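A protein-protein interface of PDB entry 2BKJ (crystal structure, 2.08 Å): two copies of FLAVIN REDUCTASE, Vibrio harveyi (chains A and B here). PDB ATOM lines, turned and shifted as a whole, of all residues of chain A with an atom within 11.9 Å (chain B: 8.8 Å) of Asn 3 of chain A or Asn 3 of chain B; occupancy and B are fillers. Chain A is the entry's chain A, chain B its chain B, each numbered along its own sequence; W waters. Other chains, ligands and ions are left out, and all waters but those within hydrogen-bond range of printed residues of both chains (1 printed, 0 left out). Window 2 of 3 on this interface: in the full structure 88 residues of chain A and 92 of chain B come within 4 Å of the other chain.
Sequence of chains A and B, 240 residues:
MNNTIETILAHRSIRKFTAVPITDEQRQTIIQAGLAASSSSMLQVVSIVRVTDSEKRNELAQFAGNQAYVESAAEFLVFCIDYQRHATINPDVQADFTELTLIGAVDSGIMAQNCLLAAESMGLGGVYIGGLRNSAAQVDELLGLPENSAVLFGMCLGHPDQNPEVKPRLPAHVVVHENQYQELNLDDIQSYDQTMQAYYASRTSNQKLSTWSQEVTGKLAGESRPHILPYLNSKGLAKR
ND2 of Asn 2 of chain A lies within hydrogen-bond range of OG of Ser 121 of chain B (3.3 Å).
The side-chain hydroxyl of Thr 7 of chain B sits at hydrogen-bond distance from the side-chain hydroxyl of Thr 4 of chain A.
The side-chain hydroxyl (OG1) of Thr 4 of chain B sits at hydrogen-bond distance from the side-chain hydroxyl (OG1) of Thr 7 of chain A, at 3.4 Å.
The side-chain hydroxyl of Ser 121 of chain A lies within hydrogen-bond range of the side-chain amide oxygen of Asn 2 of chain B.
N of Thr 4 of chain A is in hydrogen-bond range of OD1 of Asn 2 of chain A (3.1 Å).
ND2 of Asn 114 of chain A lies within hydrogen-bond range of O of Ala 33 of chain A (3.0 Å).
The backbone carbonyl oxygen (O) of Leu 117 of chain A is in hydrogen-bond range of the side-chain hydroxyl (OG) of Ser 121 of chain A.
The side-chain amide oxygen (OD1) of Asn 2 of chain B is in hydrogen-bond range of the backbone NH (N) of Thr 4 of chain B (3.2 Å).
O of Asn 3 of chain B is in hydrogen-bond range of OG1 of Thr 7 of chain B, 2.9 Å away.
The side-chain hydroxyl (OG) of Ser 121 of chain B lies within hydrogen-bond range of the backbone carbonyl oxygen (O) of Leu 117 of chain B, 3.4 Å away.
O of Asn 3 of chain B touches OG1 of Thr 4 of chain A (3.6 Å).
Thr 4 of chain B touches Thr 4 of chain A (OG1 to CA, 3.3 Å).
Ile 5 of chain A touches Ser 121 of chain B (CG1 to OG, 3.6 Å).
Thr 29 of chain A touches Ile 5 of chain B (CG2 to CD1, 3.8 Å).
CG2 of Ile 8 of chain B touches O of Ala 33 of chain A, at 3.5 Å.
CB of Ala 36 of chain A touches O of Ile 8 of chain B (3.6 Å).
Asn 114 of chain A touches Leu 117 of chain B.
Leu 117 of chain B touches Leu 117 of chain A (CD1 to CD1, 3.5 Å).
Thr 4 of chain B touches Ser 121 of chain A.
Ser 121 of chain A touches Ile 5 of chain B (OG to CG1, 3.5 Å).
Printed residues of chain B within 4 Å of Ile 5 of chain A: Ser 121.
Printed residues of chain B within 4 Å of Ser 121 of chain A: Asn 2, Thr 4 and Ile 5.
Of the printed residues of chain B, Met 122 of chain A touches Ile 5.
Asn 2 of chain B touches just one residue of chain A: Ser 121 (3.3 Å).
Of chain A, only Asn 3 and Thr 4 come within 4 Å of Asn 3 of chain B.
Thr 4 of chain B touches just these residues of chain A: Asn 3, Thr 4, Thr 7 and Ser 121.
No residue of chain A comes within 4 Å of Glu 6 of chain B.
Thr 7 of chain B touches just one residue of chain A: Thr 4.
Leu 9 of chain B touches none of the printed residues of chain A.
Of chain A, only Asn 2 (3.3 Å), Thr 4 (3.6 Å) and Ile 5 (3.6 Å) come within 4 Å of Ser 121 of chain B.
The nearest residue of chain B that does not touch Asn 3 of chain A is Asn 2 of chain B (6.1 Å).
The nearest residue of chain A that does not touch Asn 3 of chain B is Asn 2 of chain A (6.0 Å).
The nearest printed residue of chain B that does not touch Met 122 of chain A is Asn 2 of chain B (4.2 Å).
Of the 12 printed residues of chain B, 8 touch a printed residue of chain A.
Printed residues of chain A that touch a printed residue of chain B: Asn 2, Asn 3, Thr 4, Ile 5, Thr 7, Thr 29, Ala 33, Ala 36, Asn 114, Leu 117, Ser 121 and Met 122.
Hydrophobic or aromatic side chains of chain A that line the printed part of chain B: Ile 5, Ala 33, Ala 36, Leu 117 and Met 122.
Along chain A the printed residues that touch a printed residue of chain B span positions 2 to 122.
Among the printed residues, 19 pairs touch across the chains.
Among the printed residues, no Asp or Glu carboxylate lies within 4 Å of a Lys or Arg side-chain nitrogen of the other chain.
Asn 3 of chain A touches Thr 4 of chain B, and with the chains exchanged Thr 4 of chain A touches Asn 3 of chain B.
Thr 4 of chain A touches Thr 7 of chain B, and with the chains exchanged Thr 7 of chain A touches Thr 4 of chain B.
Thr 4 of chain A touches Ser 121 of chain B, and with the chains exchanged Ser 121 of chain A touches Thr 4 of chain B.
Leu 117 of chain B touches its own counterpart, Leu 117 of chain A.
12 positions are printed for both chains.
Water W1 lies within hydrogen-bond range of the backbone carbonyl oxygen (O) of Ile 8 of chain B, the backbone carbonyl oxygen (O) of Ala 36 of chain A and the side-chain amide nitrogen (ND2) of Asn 114 of chain A.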
ATOM      1  N   ASN A   2      25.463 -23.960  30.229  1.00  0.00           N
ATOM      2  CA  ASN A   2      25.590 -25.146  29.329  1.00  0.00           C
ATOM      3  C   ASN A   2      26.915 -25.156  28.567  1.00  0.00           C
ATOM      4  O   ASN A   2      27.651 -24.167  28.573  1.00  0.00           O
ATOM      5  CB  ASN A   2      24.407 -25.212  28.350  1.00  0.00           C
ATOM      6  CG  ASN A   2      24.257 -23.948  27.515  1.00  0.00           C
ATOM      7  OD1 ASN A   2      25.117 -23.625  26.694  1.00  0.00           O
ATOM      8  ND2 ASN A   2      23.152 -23.235  27.714  1.00  0.00           N
ATOM      9  N   ASN A   3      27.201 -26.275  27.903  1.00  0.00           N
ATOM     10  CA  ASN A   3      28.437 -26.443  27.142  1.00  0.00           C
ATOM     11  C   ASN A   3      28.557 -25.508  25.939  1.00  0.00           C
ATOM     12  O   ASN A   3      29.658 -25.078  25.594  1.00  0.00           O
ATOM     13  CB  ASN A   3      28.590 -27.898  26.688  1.00  0.00           C
ATOM     14  N   THR A   4      27.430 -25.191  25.305  1.00  0.00           N
ATOM     15  CA  THR A   4      27.434 -24.305  24.142  1.00  0.00           C
ATOM     16  C   THR A   4      27.954 -22.914  24.499  1.00  0.00           C
ATOM     17  O   THR A   4      28.850 -22.391  23.837  1.00  0.00           O
ATOM     18  CB  THR A   4      26.030 -24.184  23.519  1.00  0.00           C
ATOM     19  OG1 THR A   4      25.561 -25.485  23.149  1.00  0.00           O
ATOM     20  CG2 THR A   4      26.064 -23.300  22.279  1.00  0.00           C
ATOM     21  N   ILE A   5      27.399 -22.330  25.557  1.00  0.00           N
ATOM     22  CA  ILE A   5      27.806 -21.002  26.004  1.00  0.00           C
ATOM     23  C   ILE A   5      29.237 -21.013  26.544  1.00  0.00           C
ATOM     24  O   ILE A   5      29.987 -20.057  26.346  1.00  0.00           O
ATOM     25  CB  ILE A   5      26.825 -20.444  27.063  1.00  0.00           C
ATOM     26  CG1 ILE A   5      25.431 -20.305  26.441  1.00  0.00           C
ATOM     27  CG2 ILE A   5      27.304 -19.089  27.578  1.00  0.00           C
ATOM     28  CD1 ILE A   5      24.358 -19.843  27.401  1.00  0.00           C
ATOM     29  N   GLU A   6      29.617 -22.111  27.193  1.00  0.00           N
ATOM     30  CA  GLU A   6      30.963 -22.250  27.741  1.00  0.00           C
ATOM     31  C   GLU A   6      31.985 -22.245  26.604  1.00  0.00           C
ATOM     32  O   GLU A   6      33.042 -21.617  26.711  1.00  0.00           O
ATOM     33  CB  GLU A   6      31.080 -23.543  28.552  1.00  0.00           C
ATOM     34  N   THR A   7      31.654 -22.932  25.512  1.00  0.00           N
ATOM     35  CA  THR A   7      32.528 -22.998  24.342  1.00  0.00           C
ATOM     36  C   THR A   7      32.663 -21.612  23.707  1.00  0.00           C
ATOM     37  O   THR A   7      33.770 -21.172  23.404  1.00  0.00           O
ATOM     38  CB  THR A   7      31.988 -23.994  23.285  1.00  0.00           C
ATOM     39  OG1 THR A   7      31.937 -25.311  23.847  1.00  0.00           O
ATOM     40  CG2 THR A   7      32.890 -24.017  22.054  1.00  0.00           C
ATOM     41  N   ILE A   8      31.537 -20.921  23.538  1.00  0.00           N
ATOM     42  CA  ILE A   8      31.526 -19.584  22.943  1.00  0.00           C
ATOM     43  C   ILE A   8      32.389 -18.594  23.727  1.00  0.00           C
ATOM     44  O   ILE A   8      33.198 -17.868  23.147  1.00  0.00           O
ATOM     45  CB  ILE A   8      30.084 -19.019  22.842  1.00  0.00           C
ATOM     46  CG1 ILE A   8      29.235 -19.888  21.910  1.00  0.00           C
ATOM     47  CG2 ILE A   8      30.109 -17.587  22.327  1.00  0.00           C
ATOM     48  CD1 ILE A   8      27.784 -19.458  21.817  1.00  0.00           C
ATOM     49  N   LEU A   9      32.231 -18.585  25.047  1.00  0.00           N
ATOM     50  CA  LEU A   9      32.979 -17.673  25.909  1.00  0.00           C
ATOM     51  C   LEU A   9      34.454 -18.023  26.095  1.00  0.00           C
ATOM     52  O   LEU A   9      35.249 -17.169  26.483  1.00  0.00           O
ATOM     53  CB  LEU A   9      32.296 -17.558  27.277  1.00  0.00           C
ATOM     54  CG  LEU A   9      30.892 -16.948  27.266  1.00  0.00           C
ATOM     55  CD1 LEU A   9      30.292 -17.018  28.659  1.00  0.00           C
ATOM     56  CD2 LEU A   9      30.946 -15.512  26.776  1.00  0.00           C
ATOM     57  N   ALA A  10      34.813 -19.273  25.812  1.00  0.00           N
ATOM     58  CA  ALA A  10      36.194 -19.731  25.958  1.00  0.00           C
ATOM     59  C   ALA A  10      37.060 -19.461  24.728  1.00  0.00           C
ATOM     60  O   ALA A  10      38.253 -19.769  24.726  1.00  0.00           O
ATOM     61  CB  ALA A  10      36.216 -21.218  26.291  1.00  0.00           C
ATOM     62  N   HIS A  11      36.468 -18.861  23.699  1.00  0.00           N
ATOM     63  CA  HIS A  11      37.185 -18.574  22.459  1.00  0.00           C
ATOM     64  C   HIS A  11      38.410 -17.662  22.534  1.00  0.00           C
ATOM     65  O   HIS A  11      38.456 -16.695  23.297  1.00  0.00           O
ATOM     66  CB  HIS A  11      36.227 -18.015  21.396  1.00  0.00           C
ATOM     67  CG  HIS A  11      36.927 -17.411  20.215  1.00  0.00           C
ATOM     68  ND1 HIS A  11      37.497 -18.172  19.217  1.00  0.00           N
ATOM     69  CD2 HIS A  11      37.210 -16.122  19.909  1.00  0.00           C
ATOM     70  CE1 HIS A  11      38.104 -17.382  18.351  1.00  0.00           C
ATOM     71  NE2 HIS A  11      37.946 -16.132  18.748  1.00  0.00           N
ATOM     72  N   THR A  29      31.504 -33.236  10.186  1.00  0.00           N
ATOM     73  CA  THR A  29      30.644 -32.642  11.208  1.00  0.00           C
ATOM     74  C   THR A  29      30.795 -31.122  11.229  1.00  0.00           C
ATOM     75  O   THR A  29      29.818 -30.397  11.424  1.00  0.00           O
ATOM     76  CB  THR A  29      30.961 -33.223  12.597  1.00  0.00           C
ATOM     77  OG1 THR A  29      30.706 -34.631  12.583  1.00  0.00           O
ATOM     78  CG2 THR A  29      30.097 -32.579  13.667  1.00  0.00           C
ATOM     79  N   ALA A  33      27.761 -28.543  10.356  1.00  0.00           N
ATOM     80  CA  ALA A  33      27.437 -27.494  11.317  1.00  0.00           C
ATOM     81  C   ALA A  33      27.296 -26.177  10.562  1.00  0.00           C
ATOM     82  O   ALA A  33      26.373 -25.397  10.812  1.00  0.00           O
ATOM     83  CB  ALA A  33      28.528 -27.386  12.364  1.00  0.00           C
ATOM     84  N   ALA A  36      24.046 -26.019   8.574  1.00  0.00           N
ATOM     85  CA  ALA A  36      22.869 -25.844   9.424  1.00  0.00           C
ATOM     86  C   ALA A  36      22.583 -24.380   9.776  1.00  0.00           C
ATOM     87  O   ALA A  36      21.577 -24.078  10.420  1.00  0.00           O
ATOM     88  CB  ALA A  36      23.017 -26.672  10.696  1.00  0.00           C
ATOM     89  N   GLN A 113      31.102 -19.047  11.449  1.00  0.00           N
ATOM     90  CA  GLN A 113      31.083 -19.081  12.906  1.00  0.00           C
ATOM     91  C   GLN A 113      30.545 -20.412  13.420  1.00  0.00           C
ATOM     92  O   GLN A 113      30.966 -20.884  14.477  1.00  0.00           O
ATOM     93  CB  GLN A 113      30.288 -17.901  13.472  1.00  0.00           C
ATOM     94  CG  GLN A 113      30.349 -17.773  14.995  1.00  0.00           C
ATOM     95  CD  GLN A 113      31.771 -17.697  15.546  1.00  0.00           C
ATOM     96  OE1 GLN A 113      32.718 -17.367  14.833  1.00  0.00           O
ATOM     97  NE2 GLN A 113      31.916 -17.999  16.827  1.00  0.00           N
ATOM     98  N   ASN A 114      29.624 -21.017  12.672  1.00  0.00           N
ATOM     99  CA  ASN A 114      29.082 -22.319  13.053  1.00  0.00           C
ATOM    100  C   ASN A 114      30.184 -23.369  12.914  1.00  0.00           C
ATOM    101  O   ASN A 114      30.325 -24.250  13.764  1.00  0.00           O
ATOM    102  CB  ASN A 114      27.886 -22.702  12.175  1.00  0.00           C
ATOM    103  CG  ASN A 114      26.552 -22.321  12.798  1.00  0.00           C
ATOM    104  OD1 ASN A 114      26.489 -21.519  13.730  1.00  0.00           O
ATOM    105  ND2 ASN A 114      25.476 -22.903  12.284  1.00  0.00           N
ATOM    106  N   LEU A 116      33.482 -22.823  13.032  1.00  0.00           N
ATOM    107  CA  LEU A 116      34.482 -22.577  14.066  1.00  0.00           C
ATOM    108  C   LEU A 116      34.043 -23.087  15.432  1.00  0.00           C
ATOM    109  O   LEU A 116      34.821 -23.740  16.128  1.00  0.00           O
ATOM    110  CB  LEU A 116      34.834 -21.088  14.142  1.00  0.00           C
ATOM    111  CG  LEU A 116      35.950 -20.710  15.125  1.00  0.00           C
ATOM    112  CD1 LEU A 116      37.210 -21.522  14.851  1.00  0.00           C
ATOM    113  CD2 LEU A 116      36.248 -19.231  15.021  1.00  0.00           C
ATOM    114  N   LEU A 117      32.800 -22.796  15.810  1.00  0.00           N
ATOM    115  CA  LEU A 117      32.270 -23.247  17.097  1.00  0.00           C
ATOM    116  C   LEU A 117      32.221 -24.767  17.178  1.00  0.00           C
ATOM    117  O   LEU A 117      32.525 -25.347  18.223  1.00  0.00           O
ATOM    118  CB  LEU A 117      30.881 -22.660  17.359  1.00  0.00           C
ATOM    119  CG  LEU A 117      30.847 -21.198  17.805  1.00  0.00           C
ATOM    120  CD1 LEU A 117      29.407 -20.737  17.955  1.00  0.00           C
ATOM    121  CD2 LEU A 117      31.602 -21.038  19.118  1.00  0.00           C
ATOM    122  N   ALA A 118      31.847 -25.409  16.072  1.00  0.00           N
ATOM    123  CA  ALA A 118      31.782 -26.869  16.018  1.00  0.00           C
ATOM    124  C   ALA A 118      33.176 -27.430  16.267  1.00  0.00           C
ATOM    125  O   ALA A 118      33.350 -28.363  17.051  1.00  0.00           O
ATOM    126  CB  ALA A 118      31.263 -27.333  14.662  1.00  0.00           C
ATOM    127  N   ALA A 119      34.169 -26.825  15.619  1.00  0.00           N
ATOM    128  CA  ALA A 119      35.559 -27.244  15.767  1.00  0.00           C
ATOM    129  C   ALA A 119      36.042 -27.042  17.201  1.00  0.00           C
ATOM    130  O   ALA A 119      36.623 -27.946  17.800  1.00  0.00           O
ATOM    131  CB  ALA A 119      36.444 -26.469  14.799  1.00  0.00           C
ATOM    132  N   GLU A 120      35.782 -25.860  17.754  1.00  0.00           N
ATOM    133  CA  GLU A 120      36.194 -25.539  19.116  1.00  0.00           C
ATOM    134  C   GLU A 120      35.569 -26.443  20.174  1.00  0.00           C
ATOM    135  O   GLU A 120      36.217 -26.772  21.169  1.00  0.00           O
ATOM    136  CB  GLU A 120      35.910 -24.068  19.428  1.00  0.00           C
ATOM    137  CG  GLU A 120      36.775 -23.104  18.622  1.00  0.00           C
ATOM    138  CD  GLU A 120      36.466 -21.640  18.890  1.00  0.00           C
ATOM    139  OE1 GLU A 120      35.311 -21.312  19.248  1.00  0.00           O
ATOM    140  OE2 GLU A 120      37.381 -20.810  18.725  1.00  0.00           O
ATOM    141  N   SER A 121      34.325 -26.868  19.952  1.00  0.00           N
ATOM    142  CA  SER A 121      33.641 -27.747  20.899  1.00  0.00           C
ATOM    143  C   SER A 121      34.276 -29.139  20.915  1.00  0.00           C
ATOM    144  O   SER A 121      34.074 -29.909  21.854  1.00  0.00           O
ATOM    145  CB  SER A 121      32.154 -27.860  20.560  1.00  0.00           C
ATOM    146  OG  SER A 121      31.948 -28.547  19.339  1.00  0.00           O
ATOM    147  N   MET A 122      35.030 -29.455  19.861  1.00  0.00           N
ATOM    148  CA  MET A 122      35.706 -30.744  19.738  1.00  0.00           C
ATOM    149  C   MET A 122      37.139 -30.666  20.256  1.00  0.00           C
ATOM    150  O   MET A 122      37.886 -31.643  20.182  1.00  0.00           O
ATOM    151  CB  MET A 122      35.723 -31.201  18.278  1.00  0.00           C
ATOM    152  CG  MET A 122      34.352 -31.326  17.649  1.00  0.00           C
ATOM    153  SD  MET A 122      34.437 -31.800  15.915  1.00  0.00           S
ATOM    154  CE  MET A 122      33.508 -33.303  15.956  1.00  0.00           C
ATOM    155  N   GLY A 123      37.520 -29.502  20.773  1.00  0.00           N
ATOM    156  CA  GLY A 123      38.863 -29.324  21.294  1.00  0.00           C
ATOM    157  C   GLY A 123      39.847 -28.780  20.274  1.00  0.00           C
ATOM    158  O   GLY A 123      41.036 -28.649  20.563  1.00  0.00           O
ATOM    159  N   ASN B   2      28.672 -33.740  21.052  1.00  0.00           N
ATOM    160  CA  ASN B   2      28.547 -32.824  22.224  1.00  0.00           C
ATOM    161  C   ASN B   2      27.322 -31.914  22.112  1.00  0.00           C
ATOM    162  O   ASN B   2      26.654 -31.882  21.076  1.00  0.00           O
ATOM    163  CB  ASN B   2      29.827 -31.994  22.398  1.00  0.00           C
ATOM    164  CG  ASN B   2      30.202 -31.215  21.147  1.00  0.00           C
ATOM    165  OD1 ASN B   2      29.503 -30.285  20.746  1.00  0.00           O
ATOM    166  ND2 ASN B   2      31.324 -31.586  20.530  1.00  0.00           N
ATOM    167  N   ASN B   3      27.044 -31.172  23.182  1.00  0.00           N
ATOM    168  CA  ASN B   3      25.896 -30.270  23.239  1.00  0.00           C
ATOM    169  C   ASN B   3      25.938 -29.103  22.252  1.00  0.00           C
ATOM    170  O   ASN B   3      24.902 -28.713  21.714  1.00  0.00           O
ATOM    171  CB  ASN B   3      25.709 -29.738  24.663  1.00  0.00           C
ATOM    172  N   THR B   4      27.123 -28.540  22.024  1.00  0.00           N
ATOM    173  CA  THR B   4      27.267 -27.415  21.100  1.00  0.00           C
ATOM    174  C   THR B   4      26.854 -27.808  19.685  1.00  0.00           C
ATOM    175  O   THR B   4      26.076 -27.108  19.039  1.00  0.00           O
ATOM    176  CB  THR B   4      28.713 -26.876  21.079  1.00  0.00           C
ATOM    177  OG1 THR B   4      29.108 -26.513  22.406  1.00  0.00           O
ATOM    178  CG2 THR B   4      28.819 -25.651  20.174  1.00  0.00           C
ATOM    179  N   ILE B   5      27.366 -28.944  19.220  1.00  0.00           N
ATOM    180  CA  ILE B   5      27.052 -29.441  17.886  1.00  0.00           C
ATOM    181  C   ILE B   5      25.576 -29.831  17.775  1.00  0.00           C
ATOM    182  O   ILE B   5      24.947 -29.610  16.739  1.00  0.00           O
ATOM    183  CB  ILE B   5      27.975 -30.624  17.510  1.00  0.00           C
ATOM    184  CG1 ILE B   5      29.424 -30.131  17.432  1.00  0.00           C
ATOM    185  CG2 ILE B   5      27.556 -31.231  16.176  1.00  0.00           C
ATOM    186  CD1 ILE B   5      30.432 -31.215  17.147  1.00  0.00           C
ATOM    187  N   GLU B   6      25.021 -30.372  18.858  1.00  0.00           N
ATOM    188  CA  GLU B   6      23.614 -30.768  18.884  1.00  0.00           C
ATOM    189  C   GLU B   6      22.715 -29.539  18.729  1.00  0.00           C
ATOM    190  O   GLU B   6      21.724 -29.574  17.999  1.00  0.00           O
ATOM    191  CB  GLU B   6      23.287 -31.494  20.192  1.00  0.00           C
ATOM    192  N   THR B   7      23.079 -28.453  19.407  1.00  0.00           N
ATOM    193  CA  THR B   7      22.324 -27.205  19.345  1.00  0.00           C
ATOM    194  C   THR B   7      22.377 -26.613  17.934  1.00  0.00           C
ATOM    195  O   THR B   7      21.357 -26.165  17.397  1.00  0.00           O
ATOM    196  CB  THR B   7      22.874 -26.169  20.349  1.00  0.00           C
ATOM    197  OG1 THR B   7      22.819 -26.709  21.674  1.00  0.00           O
ATOM    198  CG2 THR B   7      22.059 -24.887  20.300  1.00  0.00           C
ATOM    199  N   ILE B   8      23.570 -26.626  17.341  1.00  0.00           N
ATOM    200  CA  ILE B   8      23.778 -26.103  15.993  1.00  0.00           C
ATOM    201  C   ILE B   8      22.927 -26.843  14.958  1.00  0.00           C
ATOM    202  O   ILE B   8      22.247 -26.216  14.146  1.00  0.00           O
ATOM    203  CB  ILE B   8      25.270 -26.196  15.576  1.00  0.00           C
ATOM    204  CG1 ILE B   8      26.125 -25.295  16.469  1.00  0.00           C
ATOM    205  CG2 ILE B   8      25.444 -25.789  14.120  1.00  0.00           C
ATOM    206  CD1 ILE B   8      27.608 -25.372  16.181  1.00  0.00           C
ATOM    207  N   LEU B   9      22.943 -28.171  15.017  1.00  0.00           N
ATOM    208  CA  LEU B   9      22.196 -28.995  14.072  1.00  0.00           C
ATOM    209  C   LEU B   9      20.679 -28.996  14.266  1.00  0.00           C
ATOM    210  O   LEU B   9      19.937 -29.318  13.340  1.00  0.00           O
ATOM    211  CB  LEU B   9      22.727 -30.431  14.087  1.00  0.00           C
ATOM    212  CG  LEU B   9      24.185 -30.633  13.657  1.00  0.00           C
ATOM    213  CD1 LEU B   9      24.563 -32.105  13.782  1.00  0.00           C
ATOM    214  CD2 LEU B   9      24.387 -30.150  12.227  1.00  0.00           C
ATOM    215  N   ALA B  10      20.221 -28.629  15.459  1.00  0.00           N
ATOM    216  CA  ALA B  10      18.789 -28.602  15.754  1.00  0.00           C
ATOM    217  C   ALA B  10      18.113 -27.288  15.364  1.00  0.00           C
ATOM    218  O   ALA B  10      16.911 -27.118  15.578  1.00  0.00           O
ATOM    219  CB  ALA B  10      18.554 -28.894  17.235  1.00  0.00           C
ATOM    220  N   LEU B 117      22.877 -18.745  18.727  1.00  0.00           N
ATOM    221  CA  LEU B 117      23.226 -20.055  19.276  1.00  0.00           C
ATOM    222  C   LEU B 117      23.143 -20.061  20.794  1.00  0.00           C
ATOM    223  O   LEU B 117      22.705 -21.043  21.393  1.00  0.00           O
ATOM    224  CB  LEU B 117      24.621 -20.481  18.830  1.00  0.00           C
ATOM    225  CG  LEU B 117      24.684 -21.099  17.435  1.00  0.00           C
ATOM    226  CD1 LEU B 117      26.125 -21.386  17.075  1.00  0.00           C
ATOM    227  CD2 LEU B 117      23.857 -22.376  17.389  1.00  0.00           C
ATOM    228  N   GLU B 120      19.465 -20.225  21.538  1.00  0.00           N
ATOM    229  CA  GLU B 120      18.955 -21.554  21.198  1.00  0.00           C
ATOM    230  C   GLU B 120      19.391 -22.630  22.190  1.00  0.00           C
ATOM    231  O   GLU B 120      18.665 -23.598  22.415  1.00  0.00           O
ATOM    232  CB  GLU B 120      19.378 -21.947  19.779  1.00  0.00           C
ATOM    233  CG  GLU B 120      18.735 -21.101  18.691  1.00  0.00           C
ATOM    234  CD  GLU B 120      19.211 -21.451  17.290  1.00  0.00           C
ATOM    235  OE1 GLU B 120      20.383 -21.851  17.122  1.00  0.00           O
ATOM    236  OE2 GLU B 120      18.411 -21.310  16.346  1.00  0.00           O
ATOM    237  N   SER B 121      20.573 -22.464  22.778  1.00  0.00           N
ATOM    238  CA  SER B 121      21.079 -23.432  23.748  1.00  0.00           C
ATOM    239  C   SER B 121      20.327 -23.316  25.073  1.00  0.00           C
ATOM    240  O   SER B 121      20.376 -24.227  25.898  1.00  0.00           O
ATOM    241  CB  SER B 121      22.582 -23.247  23.983  1.00  0.00           C
ATOM    242  OG  SER B 121      22.867 -22.024  24.644  1.00  0.00           O
HETATM  243  O   HOH W   1      22.660 -23.588  13.071  1.00  0.00           O
